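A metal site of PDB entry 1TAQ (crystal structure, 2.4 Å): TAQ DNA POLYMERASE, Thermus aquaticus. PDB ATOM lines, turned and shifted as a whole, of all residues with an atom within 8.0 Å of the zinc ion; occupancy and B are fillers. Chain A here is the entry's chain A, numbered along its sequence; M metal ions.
The side-chain hydroxyl (OG1) of Thr 140 sits close to the side-chain carboxylate (OD2) of Asp 18. OD1 of Asp 18 lies within hydrogen-bond range of N of His 21 (3.1 Å). The backbone carbonyl oxygen of Leu 139 sits at hydrogen-bond distance from the backbone NH of Asp 18 (3.2 Å). N of Asp 142 lies within hydrogen-bond range of OG1 of Thr 140.
CD2 of His 21 touches the zinc ion, at 3.6 Å. Leu 122 touches the zinc ion (CD1 to ZN, 3.4 Å). Thr 140 touches the zinc ion (OG1 to ZN, 3.5 Å). Leu 145 touches the zinc ion (CD1 to ZN, 3.7 Å). Seven residues have an atom within 4 Å of the zinc ion: Asp 18, His 21, Asp 119, Leu 122, Thr 140, Asp 142 and Leu 145. Along chain A the residues within 4 Å of the zinc ion span positions 18 to 145.
OD2 of Asp 18 is bound to the zinc ion. The side-chain carboxylate (OD1) of Asp 142 binds the zinc ion, 2.2 Å away. The side-chain carboxylate (OD1) of Asp 119 is bound to the zinc ion (2.2 Å).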
ATOM      1  N   VAL A  17     -20.321  27.548  12.385  1.00  0.00           N
ATOM      2  CA  VAL A  17     -19.843  26.700  13.457  1.00  0.00           C
ATOM      3  C   VAL A  17     -20.737  26.846  14.670  1.00  0.00           C
ATOM      4  O   VAL A  17     -21.159  27.947  15.015  1.00  0.00           O
ATOM      5  CB  VAL A  17     -18.375  27.049  13.832  1.00  0.00           C
ATOM      6  CG1 VAL A  17     -17.854  26.121  14.917  1.00  0.00           C
ATOM      7  CG2 VAL A  17     -17.484  26.968  12.619  1.00  0.00           C
ATOM      8  N   ASP A  18     -21.074  25.731  15.291  1.00  0.00           N
ATOM      9  CA  ASP A  18     -21.902  25.764  16.486  1.00  0.00           C
ATOM     10  C   ASP A  18     -20.956  25.892  17.651  1.00  0.00           C
ATOM     11  O   ASP A  18     -20.784  24.950  18.425  1.00  0.00           O
ATOM     12  CB  ASP A  18     -22.709  24.468  16.600  1.00  0.00           C
ATOM     13  CG  ASP A  18     -23.653  24.480  17.804  1.00  0.00           C
ATOM     14  OD1 ASP A  18     -23.799  25.511  18.489  1.00  0.00           O
ATOM     15  OD2 ASP A  18     -24.279  23.437  18.054  1.00  0.00           O
ATOM     16  N   GLY A  19     -20.366  27.075  17.804  1.00  0.00           N
ATOM     17  CA  GLY A  19     -19.428  27.297  18.888  1.00  0.00           C
ATOM     18  C   GLY A  19     -19.966  26.834  20.216  1.00  0.00           C
ATOM     19  O   GLY A  19     -19.271  26.164  20.992  1.00  0.00           O
ATOM     20  N   HIS A  20     -21.236  27.120  20.444  1.00  0.00           N
ATOM     21  CA  HIS A  20     -21.888  26.756  21.689  1.00  0.00           C
ATOM     22  C   HIS A  20     -21.892  25.261  21.983  1.00  0.00           C
ATOM     23  O   HIS A  20     -21.421  24.828  23.032  1.00  0.00           O
ATOM     24  CB  HIS A  20     -23.303  27.283  21.738  1.00  0.00           C
ATOM     25  CG  HIS A  20     -23.926  27.206  23.099  1.00  0.00           C
ATOM     26  ND1 HIS A  20     -23.201  27.418  24.254  1.00  0.00           N
ATOM     27  CD2 HIS A  20     -25.189  26.941  23.490  1.00  0.00           C
ATOM     28  CE1 HIS A  20     -24.004  27.294  25.295  1.00  0.00           C
ATOM     29  NE2 HIS A  20     -25.213  27.011  24.861  1.00  0.00           N
ATOM     30  N   HIS A  21     -22.429  24.464  21.069  1.00  0.00           N
ATOM     31  CA  HIS A  21     -22.478  23.045  21.363  1.00  0.00           C
ATOM     32  C   HIS A  21     -21.199  22.322  21.105  1.00  0.00           C
ATOM     33  O   HIS A  21     -20.992  21.233  21.640  1.00  0.00           O
ATOM     34  CB  HIS A  21     -23.694  22.370  20.724  1.00  0.00           C
ATOM     35  CG  HIS A  21     -24.999  22.841  21.319  1.00  0.00           C
ATOM     36  ND1 HIS A  21     -25.360  22.554  22.618  1.00  0.00           N
ATOM     37  CD2 HIS A  21     -25.975  23.632  20.819  1.00  0.00           C
ATOM     38  CE1 HIS A  21     -26.506  23.160  22.895  1.00  0.00           C
ATOM     39  NE2 HIS A  21     -26.897  23.822  21.826  1.00  0.00           N
ATOM     40  N   LEU A  22     -20.292  22.941  20.362  1.00  0.00           N
ATOM     41  CA  LEU A  22     -19.008  22.317  20.125  1.00  0.00           C
ATOM     42  C   LEU A  22     -18.227  22.491  21.409  1.00  0.00           C
ATOM     43  O   LEU A  22     -17.614  21.559  21.890  1.00  0.00           O
ATOM     44  CB  LEU A  22     -18.259  22.976  18.969  1.00  0.00           C
ATOM     45  CG  LEU A  22     -18.908  23.057  17.590  1.00  0.00           C
ATOM     46  CD1 LEU A  22     -17.803  23.270  16.571  1.00  0.00           C
ATOM     47  CD2 LEU A  22     -19.694  21.792  17.271  1.00  0.00           C
ATOM     48  N   VAL A  65     -21.322  30.578  15.934  1.00  0.00           N
ATOM     49  CA  VAL A  65     -22.474  30.977  16.740  1.00  0.00           C
ATOM     50  C   VAL A  65     -22.356  30.509  18.203  1.00  0.00           C
ATOM     51  O   VAL A  65     -21.951  29.371  18.479  1.00  0.00           O
ATOM     52  CB  VAL A  65     -23.793  30.464  16.103  1.00  0.00           C
ATOM     53  CG1 VAL A  65     -24.987  30.716  17.024  1.00  0.00           C
ATOM     54  CG2 VAL A  65     -23.999  31.143  14.743  1.00  0.00           C
ATOM     55  N   GLU A 117     -31.156  31.298  21.315  1.00  0.00           N
ATOM     56  CA  GLU A 117     -30.368  30.089  21.549  1.00  0.00           C
ATOM     57  C   GLU A 117     -29.556  29.741  20.313  1.00  0.00           C
ATOM     58  O   GLU A 117     -30.111  29.616  19.225  1.00  0.00           O
ATOM     59  CB  GLU A 117     -31.268  28.901  21.896  1.00  0.00           C
ATOM     60  CG  GLU A 117     -32.193  29.148  23.067  1.00  0.00           C
ATOM     61  CD  GLU A 117     -33.240  28.058  23.220  1.00  0.00           C
ATOM     62  OE1 GLU A 117     -33.651  27.472  22.186  1.00  0.00           O
ATOM     63  OE2 GLU A 117     -33.662  27.799  24.364  1.00  0.00           O
ATOM     64  N   ALA A 118     -28.264  29.542  20.513  1.00  0.00           N
ATOM     65  CA  ALA A 118     -27.340  29.203  19.445  1.00  0.00           C
ATOM     66  C   ALA A 118     -27.961  28.522  18.222  1.00  0.00           C
ATOM     67  O   ALA A 118     -27.840  29.003  17.109  1.00  0.00           O
ATOM     68  CB  ALA A 118     -26.224  28.353  20.007  1.00  0.00           C
ATOM     69  N   ASP A 119     -28.667  27.406  18.444  1.00  0.00           N
ATOM     70  CA  ASP A 119     -29.291  26.652  17.361  1.00  0.00           C
ATOM     71  C   ASP A 119     -30.244  27.452  16.458  1.00  0.00           C
ATOM     72  O   ASP A 119     -30.236  27.259  15.245  1.00  0.00           O
ATOM     73  CB  ASP A 119     -30.013  25.413  17.892  1.00  0.00           C
ATOM     74  CG  ASP A 119     -29.071  24.240  18.187  1.00  0.00           C
ATOM     75  OD1 ASP A 119     -27.831  24.433  18.312  1.00  0.00           O
ATOM     76  OD2 ASP A 119     -29.575  23.116  18.301  1.00  0.00           O
ATOM     77  N   ASP A 120     -31.075  28.307  17.044  1.00  0.00           N
ATOM     78  CA  ASP A 120     -32.010  29.132  16.274  1.00  0.00           C
ATOM     79  C   ASP A 120     -31.261  30.094  15.335  1.00  0.00           C
ATOM     80  O   ASP A 120     -31.612  30.248  14.169  1.00  0.00           O
ATOM     81  CB  ASP A 120     -32.928  29.923  17.213  1.00  0.00           C
ATOM     82  CG  ASP A 120     -34.055  29.072  17.793  1.00  0.00           C
ATOM     83  OD1 ASP A 120     -34.499  28.150  17.093  1.00  0.00           O
ATOM     84  OD2 ASP A 120     -34.479  29.345  18.940  1.00  0.00           O
ATOM     85  N   LEU A 122     -28.245  29.668  14.359  1.00  0.00           N
ATOM     86  CA  LEU A 122     -27.555  28.802  13.381  1.00  0.00           C
ATOM     87  C   LEU A 122     -28.469  28.433  12.231  1.00  0.00           C
ATOM     88  O   LEU A 122     -28.126  28.630  11.063  1.00  0.00           O
ATOM     89  CB  LEU A 122     -27.081  27.512  14.034  1.00  0.00           C
ATOM     90  CG  LEU A 122     -25.833  27.502  14.911  1.00  0.00           C
ATOM     91  CD1 LEU A 122     -25.851  26.253  15.755  1.00  0.00           C
ATOM     92  CD2 LEU A 122     -24.580  27.517  14.071  1.00  0.00           C
ATOM     93  N   ALA A 123     -29.631  27.898  12.566  1.00  0.00           N
ATOM     94  CA  ALA A 123     -30.610  27.496  11.570  1.00  0.00           C
ATOM     95  C   ALA A 123     -30.962  28.680  10.673  1.00  0.00           C
ATOM     96  O   ALA A 123     -31.019  28.558   9.448  1.00  0.00           O
ATOM     97  CB  ALA A 123     -31.854  26.973  12.255  1.00  0.00           C
ATOM     98  N   ILE A 138     -22.667  23.427   7.940  1.00  0.00           N
ATOM     99  CA  ILE A 138     -22.722  23.657   9.373  1.00  0.00           C
ATOM    100  C   ILE A 138     -21.908  22.639  10.157  1.00  0.00           C
ATOM    101  O   ILE A 138     -22.209  21.459  10.115  1.00  0.00           O
ATOM    102  CB  ILE A 138     -24.159  23.548   9.907  1.00  0.00           C
ATOM    103  CG1 ILE A 138     -25.112  24.287   8.967  1.00  0.00           C
ATOM    104  CG2 ILE A 138     -24.259  24.131  11.312  1.00  0.00           C
ATOM    105  CD1 ILE A 138     -26.549  24.228   9.451  1.00  0.00           C
ATOM    106  N   LEU A 139     -20.877  23.092  10.867  1.00  0.00           N
ATOM    107  CA  LEU A 139     -20.079  22.167  11.660  1.00  0.00           C
ATOM    108  C   LEU A 139     -20.763  21.995  12.994  1.00  0.00           C
ATOM    109  O   LEU A 139     -20.721  22.879  13.859  1.00  0.00           O
ATOM    110  CB  LEU A 139     -18.664  22.689  11.888  1.00  0.00           C
ATOM    111  CG  LEU A 139     -17.606  21.713  12.450  1.00  0.00           C
ATOM    112  CD1 LEU A 139     -16.290  22.464  12.674  1.00  0.00           C
ATOM    113  CD2 LEU A 139     -18.047  21.058  13.742  1.00  0.00           C
ATOM    114  N   THR A 140     -21.356  20.820  13.192  1.00  0.00           N
ATOM    115  CA  THR A 140     -22.054  20.504  14.426  1.00  0.00           C
ATOM    116  C   THR A 140     -22.182  19.007  14.592  1.00  0.00           C
ATOM    117  O   THR A 140     -22.002  18.231  13.647  1.00  0.00           O
ATOM    118  CB  THR A 140     -23.464  21.116  14.477  1.00  0.00           C
ATOM    119  OG1 THR A 140     -24.003  20.963  15.804  1.00  0.00           O
ATOM    120  CG2 THR A 140     -24.386  20.410  13.490  1.00  0.00           C
ATOM    121  N   ALA A 141     -22.445  18.611  15.833  1.00  0.00           N
ATOM    122  CA  ALA A 141     -22.662  17.224  16.202  1.00  0.00           C
ATOM    123  C   ALA A 141     -24.135  17.060  16.537  1.00  0.00           C
ATOM    124  O   ALA A 141     -24.749  16.057  16.160  1.00  0.00           O
ATOM    125  CB  ALA A 141     -21.795  16.869  17.408  1.00  0.00           C
ATOM    126  N   ASP A 142     -24.711  18.048  17.232  1.00  0.00           N
ATOM    127  CA  ASP A 142     -26.118  17.972  17.615  1.00  0.00           C
ATOM    128  C   ASP A 142     -26.929  17.708  16.348  1.00  0.00           C
ATOM    129  O   ASP A 142     -26.868  18.457  15.379  1.00  0.00           O
ATOM    130  CB  ASP A 142     -26.564  19.227  18.385  1.00  0.00           C
ATOM    131  CG  ASP A 142     -27.172  20.307  17.503  1.00  0.00           C
ATOM    132  OD1 ASP A 142     -26.418  21.064  16.891  1.00  0.00           O
ATOM    133  OD2 ASP A 142     -28.420  20.399  17.444  1.00  0.00           O
ATOM    134  N   LYS A 143     -27.618  16.566  16.380  1.00  0.00           N
ATOM    135  CA  LYS A 143     -28.414  16.085  15.263  1.00  0.00           C
ATOM    136  C   LYS A 143     -29.615  16.920  14.837  1.00  0.00           C
ATOM    137  O   LYS A 143     -29.987  16.869  13.677  1.00  0.00           O
ATOM    138  CB  LYS A 143     -28.810  14.631  15.511  1.00  0.00           C
ATOM    139  CG  LYS A 143     -27.612  13.767  15.874  1.00  0.00           C
ATOM    140  CD  LYS A 143     -27.857  12.279  15.620  1.00  0.00           C
ATOM    141  CE  LYS A 143     -28.978  11.717  16.488  1.00  0.00           C
ATOM    142  NZ  LYS A 143     -29.295  10.296  16.144  1.00  0.00           N
ATOM    143  N   ASP A 144     -30.172  17.726  15.733  1.00  0.00           N
ATOM    144  CA  ASP A 144     -31.339  18.557  15.399  1.00  0.00           C
ATOM    145  C   ASP A 144     -31.196  19.230  14.026  1.00  0.00           C
ATOM    146  O   ASP A 144     -32.076  19.134  13.176  1.00  0.00           O
ATOM    147  CB  ASP A 144     -31.567  19.642  16.466  1.00  0.00           C
ATOM    148  CG  ASP A 144     -31.742  19.078  17.867  1.00  0.00           C
ATOM    149  OD1 ASP A 144     -32.751  18.392  18.135  1.00  0.00           O
ATOM    150  OD2 ASP A 144     -30.872  19.352  18.728  1.00  0.00           O
ATOM    151  N   LEU A 145     -30.044  19.847  13.788  1.00  0.00           N
ATOM    152  CA  LEU A 145     -29.781  20.567  12.537  1.00  0.00           C
ATOM    153  C   LEU A 145     -29.860  19.717  11.263  1.00  0.00           C
ATOM    154  O   LEU A 145     -29.751  20.232  10.146  1.00  0.00           O
ATOM    155  CB  LEU A 145     -28.411  21.264  12.611  1.00  0.00           C
ATOM    156  CG  LEU A 145     -28.174  22.164  13.823  1.00  0.00           C
ATOM    157  CD1 LEU A 145     -26.837  22.886  13.661  1.00  0.00           C
ATOM    158  CD2 LEU A 145     -29.311  23.182  13.993  1.00  0.00           C
ATOM    159  N   VAL A 248     -35.667  25.252  16.057  1.00  0.00           N
ATOM    160  CA  VAL A 248     -34.817  25.517  14.921  1.00  0.00           C
ATOM    161  C   VAL A 248     -35.686  26.347  13.986  1.00  0.00           C
ATOM    162  O   VAL A 248     -36.002  25.923  12.878  1.00  0.00           O
ATOM    163  CB  VAL A 248     -34.412  24.211  14.234  1.00  0.00           C
ATOM    164  CG1 VAL A 248     -33.440  23.435  15.102  1.00  0.00           C
ATOM    165  CG2 VAL A 248     -35.644  23.371  13.957  1.00  0.00           C
HETATM  166 ZN    ZN M   1     -26.284  23.222  17.271  1.00  0.00          ZN
